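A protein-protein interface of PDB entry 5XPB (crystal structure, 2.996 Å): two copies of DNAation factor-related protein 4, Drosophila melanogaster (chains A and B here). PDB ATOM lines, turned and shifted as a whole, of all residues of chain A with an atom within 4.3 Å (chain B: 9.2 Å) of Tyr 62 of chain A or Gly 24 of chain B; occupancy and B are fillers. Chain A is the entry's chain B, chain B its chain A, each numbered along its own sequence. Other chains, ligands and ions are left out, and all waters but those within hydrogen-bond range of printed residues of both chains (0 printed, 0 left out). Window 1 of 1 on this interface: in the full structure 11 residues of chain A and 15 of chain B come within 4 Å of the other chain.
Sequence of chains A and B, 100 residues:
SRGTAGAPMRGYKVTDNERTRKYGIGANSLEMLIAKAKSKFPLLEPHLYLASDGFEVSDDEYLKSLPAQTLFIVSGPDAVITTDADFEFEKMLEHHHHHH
SD of Met 9 of chain B is in hydrogen-bond range of N of Ala 27 of chain B (3.3 Å).
The backbone NH (N) of Gln 69 of chain B is in hydrogen-bond range of the backbone carbonyl oxygen (O) of Gly 11 of chain B, at 2.7 Å.
N of Tyr 12 of chain B is in hydrogen-bond range of O of Ile 25 of chain B, 2.9 Å away.
The backbone NH (N) of Lys 13 of chain B lies within hydrogen-bond range of the backbone carbonyl oxygen (O) of Thr 70 of chain B, 3.0 Å away.
The backbone carbonyl oxygen (O) of Tyr 23 of chain B is in hydrogen-bond range of the backbone NH (N) of Val 14 of chain B (3.1 Å).
The side-chain hydroxyl of Ser 58 of chain A is in hydrogen-bond range of the side-chain carboxylate of Asp 59 of chain A (2.9 Å).
Printed residues of chain B within 4 Å of Leu 50 of chain A: Lys 13 (3.4 Å).
Val 57 of chain A touches none of the printed residues of chain B.
Tyr 62 of chain A touches just these residues of chain B: Gly 11, Tyr 12, Lys 13, Gly 24, Ile 25, Gly 26 and Gln 69.
Of chain B, only Gly 11 and Gln 69 come within 4 Å of Ser 65 of chain A.
Of the printed residues of chain A, Gly 11 of chain B touches Tyr 62 (3.7 Å) and Ser 65 (3.5 Å).
Gly 24 of chain B touches just these residues of chain A: Glu 56, Ser 58, Asp 59 and Tyr 62.
Ala 37 of chain B touches none of the printed residues of chain A.
The nearest printed residue of chain A that does not touch Gly 24 of chain B is Val 57 of chain A (4.6 Å).
OH of Tyr 62 of chain A is in hydrogen-bond range of NZ of Lys 13 of chain B (2.9 Å).
The side-chain carboxylate of Glu 56 of chain A lies within salt-bridge range of the guanidinium group of Arg 21 of chain B (3.4 Å).
The backbone carbonyl oxygen (O) of Lys 22 of chain B lies within hydrogen-bond range of the backbone NH (N) of Glu 56 of chain A.
The backbone NH of Gly 24 of chain B is in hydrogen-bond range of the backbone carbonyl oxygen of Glu 56 of chain A, 2.8 Å away.
The backbone carbonyl oxygen (O) of Gly 24 of chain B sits close to the backbone NH (N) of Ser 58 of chain A.
The backbone NH (N) of Gly 26 of chain B sits at hydrogen-bond distance from the side-chain carboxylate (OD2) of Asp 59 of chain A (3.3 Å).
The side-chain amino group (NZ) of Lys 36 of chain B lies within salt-bridge range of the side-chain carboxylate (OD2) of Asp 59 of chain A (3.1 Å).
OE1 of Glu 61 of chain A is in salt-bridge range of NZ of Lys 36 of chain B, at 2.9 Å.
The side-chain amide oxygen of Gln 69 of chain B is in hydrogen-bond range of the side-chain hydroxyl of Tyr 62 of chain A, at 2.6 Å.
The side-chain carboxylate (OD1) of Asp 59 of chain A sits close to the backbone carbonyl oxygen (O) of Gly 24 of chain B, 3.4 Å away.
The side-chain amide nitrogen (NE2) of Gln 69 of chain B sits close to the side-chain hydroxyl (OG) of Ser 65 of chain A, 2.3 Å away.
No position is printed for both chains.
Of the 24 pairs that touch across the chains among the printed residues, none has its exchanged pair printed and touching as well.
Hydrophobic or aromatic side chains of chain A that line the printed part of chain B: Leu 50 and Tyr 62.
Hydrophobic or aromatic side chains of chain B within 4 Å of the printed part of chain A: Met 9 and Tyr 23.
Among the printed residues, 24 pairs touch across the chains.
Leu 50 of chain A touches Lys 13 of chain B.
Tyr 23 of chain B touches Ser 58 of chain A (CD1 to CB, 3.7 Å).
CB of Ser 58 of chain A touches NZ of Lys 40 of chain B (3.9 Å).
Asp 59 of chain A touches Ile 25 of chain B.
Met 9 of chain B touches Glu 61 of chain A.
CA of Gly 26 of chain B touches CB of Glu 61 of chain A, at 3.9 Å.
CD2 of Tyr 62 of chain A touches CA of Gly 11 of chain B, 3.7 Å away.
Tyr 12 of chain B touches Tyr 62 of chain A (O to CE2, 3.6 Å).
Ile 25 of chain B touches Tyr 62 of chain A (N to CD2, 3.4 Å).
Ser 65 of chain A touches Gly 11 of chain B (OG to CA, 3.5 Å).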
ATOM      1  N   LEU A  50     -14.339 -10.704  11.009  1.00  0.00           N
ATOM      2  CA  LEU A  50     -15.603 -10.867  11.695  1.00  0.00           C
ATOM      3  C   LEU A  50     -16.134  -9.493  12.058  1.00  0.00           C
ATOM      4  O   LEU A  50     -15.413  -8.666  12.621  1.00  0.00           O
ATOM      5  CB  LEU A  50     -15.426 -11.735  12.941  1.00  0.00           C
ATOM      6  CG  LEU A  50     -14.828 -13.117  12.648  1.00  0.00           C
ATOM      7  CD1 LEU A  50     -14.498 -13.844  13.943  1.00  0.00           C
ATOM      8  CD2 LEU A  50     -15.734 -13.974  11.785  1.00  0.00           C
ATOM      9  N   GLU A  56      -9.267 -11.348  11.809  1.00  0.00           N
ATOM     10  CA  GLU A  56      -9.097 -11.739  10.419  1.00  0.00           C
ATOM     11  C   GLU A  56      -9.333 -13.242  10.279  1.00  0.00           C
ATOM     12  O   GLU A  56      -8.728 -14.048  10.987  1.00  0.00           O
ATOM     13  CB  GLU A  56      -7.691 -11.367   9.929  1.00  0.00           C
ATOM     14  CG  GLU A  56      -7.438 -11.705   8.452  1.00  0.00           C
ATOM     15  CD  GLU A  56      -6.028 -11.378   7.957  1.00  0.00           C
ATOM     16  OE1 GLU A  56      -5.495 -12.199   7.158  1.00  0.00           O
ATOM     17  OE2 GLU A  56      -5.459 -10.328   8.372  1.00  0.00           O
ATOM     18  N   VAL A  57     -10.211 -13.623   9.362  1.00  0.00           N
ATOM     19  CA  VAL A  57     -10.356 -15.028   9.016  1.00  0.00           C
ATOM     20  C   VAL A  57      -9.099 -15.382   8.232  1.00  0.00           C
ATOM     21  O   VAL A  57      -9.025 -15.121   7.028  1.00  0.00           O
ATOM     22  CB  VAL A  57     -11.646 -15.269   8.203  1.00  0.00           C
ATOM     23  CG1 VAL A  57     -11.678 -16.669   7.579  1.00  0.00           C
ATOM     24  CG2 VAL A  57     -12.888 -14.994   9.046  1.00  0.00           C
ATOM     25  N   SER A  58      -8.107 -15.983   8.896  1.00  0.00           N
ATOM     26  CA  SER A  58      -6.769 -16.080   8.316  1.00  0.00           C
ATOM     27  C   SER A  58      -6.558 -17.316   7.446  1.00  0.00           C
ATOM     28  O   SER A  58      -5.768 -17.260   6.491  1.00  0.00           O
ATOM     29  CB  SER A  58      -5.715 -16.060   9.424  1.00  0.00           C
ATOM     30  OG  SER A  58      -5.902 -17.166  10.285  1.00  0.00           O
ATOM     31  N   ASP A  59      -7.197 -18.439   7.768  1.00  0.00           N
ATOM     32  CA  ASP A  59      -7.086 -19.658   6.972  1.00  0.00           C
ATOM     33  C   ASP A  59      -8.476 -20.236   6.743  1.00  0.00           C
ATOM     34  O   ASP A  59      -9.448 -19.866   7.402  1.00  0.00           O
ATOM     35  CB  ASP A  59      -6.145 -20.728   7.588  1.00  0.00           C
ATOM     36  CG  ASP A  59      -6.394 -20.972   9.070  1.00  0.00           C
ATOM     37  OD1 ASP A  59      -6.572 -19.990   9.832  1.00  0.00           O
ATOM     38  OD2 ASP A  59      -6.405 -22.162   9.470  1.00  0.00           O
ATOM     39  N   ASP A  60      -8.561 -21.142   5.767  1.00  0.00           N
ATOM     40  CA  ASP A  60      -9.837 -21.754   5.427  1.00  0.00           C
ATOM     41  C   ASP A  60     -10.391 -22.544   6.609  1.00  0.00           C
ATOM     42  O   ASP A  60     -11.607 -22.534   6.846  1.00  0.00           O
ATOM     43  CB  ASP A  60      -9.631 -22.635   4.191  1.00  0.00           C
ATOM     44  CG  ASP A  60     -10.888 -23.395   3.736  1.00  0.00           C
ATOM     45  OD1 ASP A  60     -12.014 -23.142   4.225  1.00  0.00           O
ATOM     46  OD2 ASP A  60     -10.749 -24.273   2.854  1.00  0.00           O
ATOM     47  N   GLU A  61      -9.521 -23.193   7.397  1.00  0.00           N
ATOM     48  CA  GLU A  61     -10.032 -23.977   8.520  1.00  0.00           C
ATOM     49  C   GLU A  61     -10.759 -23.093   9.519  1.00  0.00           C
ATOM     50  O   GLU A  61     -11.799 -23.494  10.052  1.00  0.00           O
ATOM     51  CB  GLU A  61      -8.927 -24.772   9.198  1.00  0.00           C
ATOM     52  CG  GLU A  61      -8.385 -25.898   8.349  1.00  0.00           C
ATOM     53  CD  GLU A  61      -7.305 -25.407   7.437  1.00  0.00           C
ATOM     54  OE1 GLU A  61      -6.494 -24.572   7.908  1.00  0.00           O
ATOM     55  OE2 GLU A  61      -7.267 -25.853   6.269  1.00  0.00           O
ATOM     56  N   TYR A  62     -10.225 -21.905   9.819  1.00  0.00           N
ATOM     57  CA  TYR A  62     -10.971 -21.036  10.719  1.00  0.00           C
ATOM     58  C   TYR A  62     -12.311 -20.605  10.116  1.00  0.00           C
ATOM     59  O   TYR A  62     -13.264 -20.360  10.861  1.00  0.00           O
ATOM     60  CB  TYR A  62     -10.161 -19.809  11.073  1.00  0.00           C
ATOM     61  CG  TYR A  62     -10.871 -18.983  12.095  1.00  0.00           C
ATOM     62  CD1 TYR A  62     -11.504 -17.803  11.767  1.00  0.00           C
ATOM     63  CD2 TYR A  62     -10.985 -19.442  13.381  1.00  0.00           C
ATOM     64  CE1 TYR A  62     -12.171 -17.066  12.722  1.00  0.00           C
ATOM     65  CE2 TYR A  62     -11.637 -18.712  14.343  1.00  0.00           C
ATOM     66  CZ  TYR A  62     -12.228 -17.530  14.016  1.00  0.00           C
ATOM     67  OH  TYR A  62     -12.873 -16.842  15.017  1.00  0.00           O
ATOM     68  N   LEU A  63     -12.417 -20.506   8.780  1.00  0.00           N
ATOM     69  CA  LEU A  63     -13.708 -20.179   8.162  1.00  0.00           C
ATOM     70  C   LEU A  63     -14.740 -21.283   8.405  1.00  0.00           C
ATOM     71  O   LEU A  63     -15.908 -20.990   8.687  1.00  0.00           O
ATOM     72  CB  LEU A  63     -13.561 -19.910   6.665  1.00  0.00           C
ATOM     73  CG  LEU A  63     -14.900 -19.719   5.939  1.00  0.00           C
ATOM     74  CD1 LEU A  63     -15.501 -18.351   6.286  1.00  0.00           C
ATOM     75  CD2 LEU A  63     -14.792 -19.936   4.420  1.00  0.00           C
ATOM     76  N   LYS A  64     -14.363 -22.555   8.226  1.00  0.00           N
ATOM     77  CA  LYS A  64     -15.332 -23.596   8.566  1.00  0.00           C
ATOM     78  C   LYS A  64     -15.518 -23.773  10.071  1.00  0.00           C
ATOM     79  O   LYS A  64     -16.493 -24.408  10.494  1.00  0.00           O
ATOM     80  CB  LYS A  64     -14.965 -24.941   7.948  1.00  0.00           C
ATOM     81  CG  LYS A  64     -15.277 -25.056   6.491  1.00  0.00           C
ATOM     82  CD  LYS A  64     -14.104 -24.959   5.579  1.00  0.00           C
ATOM     83  CE  LYS A  64     -14.410 -25.775   4.317  1.00  0.00           C
ATOM     84  NZ  LYS A  64     -13.370 -25.679   3.266  1.00  0.00           N
ATOM     85  N   SER A  65     -14.615 -23.232  10.888  1.00  0.00           N
ATOM     86  CA  SER A  65     -14.906 -23.101  12.307  1.00  0.00           C
ATOM     87  C   SER A  65     -16.227 -22.386  12.548  1.00  0.00           C
ATOM     88  O   SER A  65     -16.948 -22.713  13.495  1.00  0.00           O
ATOM     89  CB  SER A  65     -13.781 -22.340  13.007  1.00  0.00           C
ATOM     90  OG  SER A  65     -14.297 -21.555  14.076  1.00  0.00           O
ATOM     91  N   LEU A  66     -16.557 -21.388  11.697  1.00  0.00           N
ATOM     92  CA  LEU A  66     -17.646 -20.455  11.959  1.00  0.00           C
ATOM     93  C   LEU A  66     -19.012 -21.000  11.543  1.00  0.00           C
ATOM     94  O   LEU A  66     -19.120 -21.759  10.576  1.00  0.00           O
ATOM     95  CB  LEU A  66     -17.404 -19.154  11.218  1.00  0.00           C
ATOM     96  CG  LEU A  66     -16.090 -18.459  11.497  1.00  0.00           C
ATOM     97  CD1 LEU A  66     -15.762 -17.512  10.346  1.00  0.00           C
ATOM     98  CD2 LEU A  66     -16.174 -17.742  12.828  1.00  0.00           C
ATOM     99  N   MET B   9     -10.487 -30.325  13.549  1.00  0.00           N
ATOM    100  CA  MET B   9     -10.018 -28.953  13.430  1.00  0.00           C
ATOM    101  C   MET B   9     -10.975 -28.012  14.157  1.00  0.00           C
ATOM    102  O   MET B   9     -12.191 -28.116  13.996  1.00  0.00           O
ATOM    103  CB  MET B   9      -9.852 -28.566  11.963  1.00  0.00           C
ATOM    104  CG  MET B   9      -9.031 -27.289  11.772  1.00  0.00           C
ATOM    105  SD  MET B   9      -7.270 -27.620  11.673  1.00  0.00           S
ATOM    106  CE  MET B   9      -7.313 -28.952  10.473  1.00  0.00           C
ATOM    107  N   ARG B  10     -10.437 -27.120  14.986  1.00  0.00           N
ATOM    108  CA  ARG B  10     -11.273 -26.193  15.734  1.00  0.00           C
ATOM    109  C   ARG B  10     -10.746 -24.772  15.588  1.00  0.00           C
ATOM    110  O   ARG B  10      -9.585 -24.555  15.245  1.00  0.00           O
ATOM    111  CB  ARG B  10     -11.328 -26.559  17.205  1.00  0.00           C
ATOM    112  CG  ARG B  10     -11.380 -28.042  17.456  1.00  0.00           C
ATOM    113  CD  ARG B  10     -11.774 -28.360  18.886  1.00  0.00           C
ATOM    114  NE  ARG B  10     -11.185 -27.441  19.847  1.00  0.00           N
ATOM    115  CZ  ARG B  10     -11.634 -27.303  21.084  1.00  0.00           C
ATOM    116  NH1 ARG B  10     -12.657 -28.037  21.487  1.00  0.00           N
ATOM    117  NH2 ARG B  10     -11.057 -26.449  21.916  1.00  0.00           N
ATOM    118  N   GLY B  11     -11.600 -23.795  15.857  1.00  0.00           N
ATOM    119  CA  GLY B  11     -11.253 -22.393  15.652  1.00  0.00           C
ATOM    120  C   GLY B  11     -10.866 -21.709  16.949  1.00  0.00           C
ATOM    121  O   GLY B  11     -11.555 -21.853  17.961  1.00  0.00           O
ATOM    122  N   TYR B  12      -9.758 -20.954  16.905  1.00  0.00           N
ATOM    123  CA  TYR B  12      -9.269 -20.218  18.068  1.00  0.00           C
ATOM    124  C   TYR B  12      -8.948 -18.763  17.705  1.00  0.00           C
ATOM    125  O   TYR B  12      -8.763 -18.419  16.538  1.00  0.00           O
ATOM    126  CB  TYR B  12      -8.029 -20.904  18.685  1.00  0.00           C
ATOM    127  CG  TYR B  12      -8.167 -22.393  19.003  1.00  0.00           C
ATOM    128  CD1 TYR B  12      -8.477 -22.818  20.296  1.00  0.00           C
ATOM    129  CD2 TYR B  12      -7.989 -23.370  18.010  1.00  0.00           C
ATOM    130  CE1 TYR B  12      -8.613 -24.161  20.601  1.00  0.00           C
ATOM    131  CE2 TYR B  12      -8.118 -24.728  18.310  1.00  0.00           C
ATOM    132  CZ  TYR B  12      -8.436 -25.113  19.615  1.00  0.00           C
ATOM    133  OH  TYR B  12      -8.571 -26.446  19.945  1.00  0.00           O
ATOM    134  N   LYS B  13      -8.900 -17.887  18.721  1.00  0.00           N
ATOM    135  CA  LYS B  13      -8.615 -16.468  18.503  1.00  0.00           C
ATOM    136  C   LYS B  13      -7.307 -16.076  19.160  1.00  0.00           C
ATOM    137  O   LYS B  13      -7.145 -16.230  20.373  1.00  0.00           O
ATOM    138  CB  LYS B  13      -9.728 -15.566  19.031  1.00  0.00           C
ATOM    139  CG  LYS B  13     -11.074 -15.794  18.333  1.00  0.00           C
ATOM    140  CD  LYS B  13     -12.221 -15.047  19.005  1.00  0.00           C
ATOM    141  CE  LYS B  13     -13.535 -15.435  18.383  1.00  0.00           C
ATOM    142  NZ  LYS B  13     -13.552 -14.898  17.007  1.00  0.00           N
ATOM    143  N   VAL B  14      -6.411 -15.493  18.356  1.00  0.00           N
ATOM    144  CA  VAL B  14      -5.040 -15.190  18.742  1.00  0.00           C
ATOM    145  C   VAL B  14      -4.751 -13.723  18.492  1.00  0.00           C
ATOM    146  O   VAL B  14      -5.046 -13.198  17.415  1.00  0.00           O
ATOM    147  CB  VAL B  14      -4.051 -16.047  17.949  1.00  0.00           C
ATOM    148  CG1 VAL B  14      -2.655 -15.765  18.434  1.00  0.00           C
ATOM    149  CG2 VAL B  14      -4.416 -17.520  18.110  1.00  0.00           C
ATOM    150  N   THR B  15      -4.090 -13.089  19.444  1.00  0.00           N
ATOM    151  CA  THR B  15      -3.662 -11.711  19.289  1.00  0.00           C
ATOM    152  C   THR B  15      -2.327 -11.574  20.015  1.00  0.00           C
ATOM    153  O   THR B  15      -1.876 -12.501  20.693  1.00  0.00           O
ATOM    154  CB  THR B  15      -4.743 -10.729  19.793  1.00  0.00           C
ATOM    155  OG1 THR B  15      -4.404  -9.387  19.428  1.00  0.00           O
ATOM    156  CG2 THR B  15      -4.900 -10.780  21.283  1.00  0.00           C
ATOM    157  N   ARG B  21      -2.838  -7.088  16.232  1.00  0.00           N
ATOM    158  CA  ARG B  21      -3.099  -8.045  15.189  1.00  0.00           C
ATOM    159  C   ARG B  21      -4.020  -9.113  15.762  1.00  0.00           C
ATOM    160  O   ARG B  21      -3.777  -9.647  16.852  1.00  0.00           O
ATOM    161  CB  ARG B  21      -1.790  -8.608  14.618  1.00  0.00           C
ATOM    162  CG  ARG B  21      -1.347  -7.859  13.314  1.00  0.00           C
ATOM    163  CD  ARG B  21      -2.425  -7.914  12.102  1.00  0.00           C
ATOM    164  NE  ARG B  21      -3.604  -7.032  12.319  1.00  0.00           N
ATOM    165  CZ  ARG B  21      -4.712  -6.937  11.566  1.00  0.00           C
ATOM    166  NH1 ARG B  21      -4.902  -7.689  10.474  1.00  0.00           N
ATOM    167  NH2 ARG B  21      -5.654  -6.086  11.953  1.00  0.00           N
ATOM    168  N   LYS B  22      -5.135  -9.337  15.076  1.00  0.00           N
ATOM    169  CA  LYS B  22      -6.173 -10.229  15.553  1.00  0.00           C
ATOM    170  C   LYS B  22      -6.469 -11.191  14.419  1.00  0.00           C
ATOM    171  O   LYS B  22      -6.755 -10.753  13.302  1.00  0.00           O
ATOM    172  CB  LYS B  22      -7.397  -9.430  16.000  1.00  0.00           C
ATOM    173  CG  LYS B  22      -7.028  -8.144  16.695  1.00  0.00           C
ATOM    174  CD  LYS B  22      -8.165  -7.511  17.504  1.00  0.00           C
ATOM    175  CE  LYS B  22      -7.622  -6.258  18.239  1.00  0.00           C
ATOM    176  NZ  LYS B  22      -8.542  -5.512  19.149  1.00  0.00           N
ATOM    177  N   TYR B  23      -6.276 -12.486  14.672  1.00  0.00           N
ATOM    178  CA  TYR B  23      -6.520 -13.537  13.690  1.00  0.00           C
ATOM    179  C   TYR B  23      -7.382 -14.633  14.293  1.00  0.00           C
ATOM    180  O   TYR B  23      -7.402 -14.831  15.511  1.00  0.00           O
ATOM    181  CB  TYR B  23      -5.247 -14.208  13.137  1.00  0.00           C
ATOM    182  CG  TYR B  23      -4.204 -13.295  12.522  1.00  0.00           C
ATOM    183  CD1 TYR B  23      -3.942 -13.341  11.151  1.00  0.00           C
ATOM    184  CD2 TYR B  23      -3.471 -12.397  13.301  1.00  0.00           C
ATOM    185  CE1 TYR B  23      -2.988 -12.511  10.574  1.00  0.00           C
ATOM    186  CE2 TYR B  23      -2.511 -11.578  12.738  1.00  0.00           C
ATOM    187  CZ  TYR B  23      -2.271 -11.638  11.376  1.00  0.00           C
ATOM    188  OH  TYR B  23      -1.321 -10.807  10.824  1.00  0.00           O
ATOM    189  N   GLY B  24      -8.155 -15.282  13.430  1.00  0.00           N
ATOM    190  CA  GLY B  24      -8.790 -16.548  13.751  1.00  0.00           C
ATOM    191  C   GLY B  24      -7.984 -17.645  13.098  1.00  0.00           C
ATOM    192  O   GLY B  24      -7.572 -17.514  11.952  1.00  0.00           O
ATOM    193  N   ILE B  25      -7.717 -18.719  13.843  1.00  0.00           N
ATOM    194  CA  ILE B  25      -6.838 -19.786  13.378  1.00  0.00           C
ATOM    195  C   ILE B  25      -7.493 -21.141  13.615  1.00  0.00           C
ATOM    196  O   ILE B  25      -7.962 -21.427  14.725  1.00  0.00           O
ATOM    197  CB  ILE B  25      -5.462 -19.754  14.066  1.00  0.00           C
ATOM    198  CG1 ILE B  25      -4.858 -18.344  14.025  1.00  0.00           C
ATOM    199  CG2 ILE B  25      -4.547 -20.759  13.397  1.00  0.00           C
ATOM    200  CD1 ILE B  25      -3.619 -18.222  14.851  1.00  0.00           C
ATOM    201  N   GLY B  26      -7.505 -21.967  12.566  1.00  0.00           N
ATOM    202  CA  GLY B  26      -7.932 -23.354  12.668  1.00  0.00           C
ATOM    203  C   GLY B  26      -6.735 -24.232  12.983  1.00  0.00           C
ATOM    204  O   GLY B  26      -5.652 -24.030  12.452  1.00  0.00           O
ATOM    205  N   ALA B  27      -6.931 -25.176  13.900  1.00  0.00           N
ATOM    206  CA  ALA B  27      -5.845 -26.012  14.398  1.00  0.00           C
ATOM    207  C   ALA B  27      -6.432 -27.225  15.103  1.00  0.00           C
ATOM    208  O   ALA B  27      -7.378 -27.099  15.887  1.00  0.00           O
ATOM    209  CB  ALA B  27      -4.934 -25.235  15.358  1.00  0.00           C
ATOM    210  N   MET B  32      -0.025 -27.368  15.803  1.00  0.00           N
ATOM    211  CA  MET B  32      -0.518 -26.701  14.601  1.00  0.00           C
ATOM    212  C   MET B  32      -0.862 -25.252  14.892  1.00  0.00           C
ATOM    213  O   MET B  32      -0.529 -24.363  14.108  1.00  0.00           O
ATOM    214  CB  MET B  32      -1.737 -27.424  14.021  1.00  0.00           C
ATOM    215  CG  MET B  32      -2.238 -26.749  12.755  1.00  0.00           C
ATOM    216  SD  MET B  32      -3.681 -27.487  11.991  1.00  0.00           S
ATOM    217  CE  MET B  32      -3.014 -29.001  11.301  1.00  0.00           C
ATOM    218  N   LEU B  33      -1.530 -25.000  16.016  1.00  0.00           N
ATOM    219  CA  LEU B  33      -1.864 -23.631  16.391  1.00  0.00           C
ATOM    220  C   LEU B  33      -0.607 -22.794  16.594  1.00  0.00           C
ATOM    221  O   LEU B  33      -0.531 -21.648  16.132  1.00  0.00           O
ATOM    222  CB  LEU B  33      -2.731 -23.641  17.652  1.00  0.00           C
ATOM    223  CG  LEU B  33      -3.318 -22.315  18.123  1.00  0.00           C
ATOM    224  CD1 LEU B  33      -3.927 -21.537  16.984  1.00  0.00           C
ATOM    225  CD2 LEU B  33      -4.383 -22.619  19.155  1.00  0.00           C
ATOM    226  N   LYS B  36       1.000 -21.930  13.204  1.00  0.00           N
ATOM    227  CA  LYS B  36       0.219 -20.925  12.493  1.00  0.00           C
ATOM    228  C   LYS B  36       0.342 -19.544  13.134  1.00  0.00           C
ATOM    229  O   LYS B  36       0.394 -18.533  12.423  1.00  0.00           O
ATOM    230  CB  LYS B  36      -1.238 -21.379  12.414  1.00  0.00           C
ATOM    231  CG  LYS B  36      -1.438 -22.722  11.680  1.00  0.00           C
ATOM    232  CD  LYS B  36      -2.854 -22.894  11.100  1.00  0.00           C
ATOM    233  CE  LYS B  36      -3.057 -24.285  10.500  1.00  0.00           C
ATOM    234  NZ  LYS B  36      -4.355 -24.448   9.793  1.00  0.00           N
ATOM    235  N   ALA B  37       0.371 -19.465  14.469  1.00  0.00           N
ATOM    236  CA  ALA B  37       0.599 -18.165  15.101  1.00  0.00           C
ATOM    237  C   ALA B  37       2.012 -17.666  14.821  1.00  0.00           C
ATOM    238  O   ALA B  37       2.233 -16.454  14.668  1.00  0.00           O
ATOM    239  CB  ALA B  37       0.354 -18.242  16.608  1.00  0.00           C
ATOM    240  N   LYS B  40       2.288 -15.794  11.527  1.00  0.00           N
ATOM    241  CA  LYS B  40       1.654 -14.486  11.487  1.00  0.00           C
ATOM    242  C   LYS B  40       2.239 -13.533  12.513  1.00  0.00           C
ATOM    243  O   LYS B  40       1.754 -12.404  12.642  1.00  0.00           O
ATOM    244  CB  LYS B  40       0.138 -14.622  11.705  1.00  0.00           C
ATOM    245  CG  LYS B  40      -0.527 -15.654  10.795  1.00  0.00           C
ATOM    246  CD  LYS B  40      -1.210 -15.029   9.600  1.00  0.00           C
ATOM    247  CE  LYS B  40      -1.673 -16.075   8.609  1.00  0.00           C
ATOM    248  NZ  LYS B  40      -2.386 -15.434   7.470  1.00  0.00           N
ATOM    249  N   PHE B  41       3.281 -13.941  13.228  1.00  0.00           N
ATOM    250  CA  PHE B  41       3.792 -13.056  14.259  1.00  0.00           C
ATOM    251  C   PHE B  41       5.312 -12.936  14.246  1.00  0.00           C
ATOM    252  O   PHE B  41       6.035 -13.862  13.848  1.00  0.00           O
ATOM    253  CB  PHE B  41       3.313 -13.509  15.641  1.00  0.00           C
ATOM    254  CG  PHE B  41       1.954 -12.985  16.005  1.00  0.00           C
ATOM    255  CD1 PHE B  41       1.822 -11.725  16.605  1.00  0.00           C
ATOM    256  CD2 PHE B  41       0.813 -13.733  15.749  1.00  0.00           C
ATOM    257  CE1 PHE B  41       0.573 -11.223  16.964  1.00  0.00           C
ATOM    258  CE2 PHE B  41      -0.435 -13.236  16.093  1.00  0.00           C
ATOM    259  CZ  PHE B  41      -0.556 -11.975  16.703  1.00  0.00           C
ATOM    260  N   ALA B  68     -14.107 -23.774  22.164  1.00  0.00           N
ATOM    261  CA  ALA B  68     -13.665 -23.166  20.916  1.00  0.00           C
ATOM    262  C   ALA B  68     -13.795 -21.633  20.960  1.00  0.00           C
ATOM    263  O   ALA B  68     -14.495 -21.052  21.804  1.00  0.00           O
ATOM    264  CB  ALA B  68     -14.433 -23.736  19.726  1.00  0.00           C
ATOM    265  N   GLN B  69     -13.069 -20.985  20.041  1.00  0.00           N
ATOM    266  CA  GLN B  69     -13.003 -19.529  19.926  1.00  0.00           C
ATOM    267  C   GLN B  69     -12.563 -18.865  21.222  1.00  0.00           C
ATOM    268  O   GLN B  69     -13.018 -17.756  21.535  1.00  0.00           O
ATOM    269  CB  GLN B  69     -14.333 -18.938  19.458  1.00  0.00           C
ATOM    270  CG  GLN B  69     -15.025 -19.751  18.394  1.00  0.00           C
ATOM    271  CD  GLN B  69     -14.395 -19.593  17.022  1.00  0.00           C
ATOM    272  OE1 GLN B  69     -13.798 -18.553  16.699  1.00  0.00           O
ATOM    273  NE2 GLN B  69     -14.533 -20.629  16.196  1.00  0.00           N
ATOM    274  N   THR B  70     -11.724 -19.550  22.004  1.00  0.00           N
ATOM    275  CA  THR B  70     -11.065 -18.907  23.141  1.00  0.00           C
ATOM    276  C   THR B  70      -9.976 -17.970  22.642  1.00  0.00           C
ATOM    277  O   THR B  70      -9.294 -18.260  21.651  1.00  0.00           O
ATOM    278  CB  THR B  70     -10.478 -19.954  24.094  1.00  0.00           C
ATOM    279  OG1 THR B  70     -11.538 -20.612  24.810  1.00  0.00           O
ATOM    280  CG2 THR B  70      -9.479 -19.344  25.072  1.00  0.00           C
ATOM    281  N   LEU B  71      -9.856 -16.813  23.294  1.00  0.00           N
ATOM    282  CA  LEU B  71      -8.864 -15.823  22.901  1.00  0.00           C
ATOM    283  C   LEU B  71      -7.562 -16.052  23.655  1.00  0.00           C
ATOM    284  O   LEU B  71      -7.543 -16.072  24.891  1.00  0.00           O
ATOM    285  CB  LEU B  71      -9.366 -14.401  23.141  1.00  0.00           C
ATOM    286  CG  LEU B  71      -8.334 -13.322  22.816  1.00  0.00           C
ATOM    287  CD1 LEU B  71      -8.091 -13.190  21.308  1.00  0.00           C
ATOM    288  CD2 LEU B  71      -8.741 -11.997  23.465  1.00  0.00           C
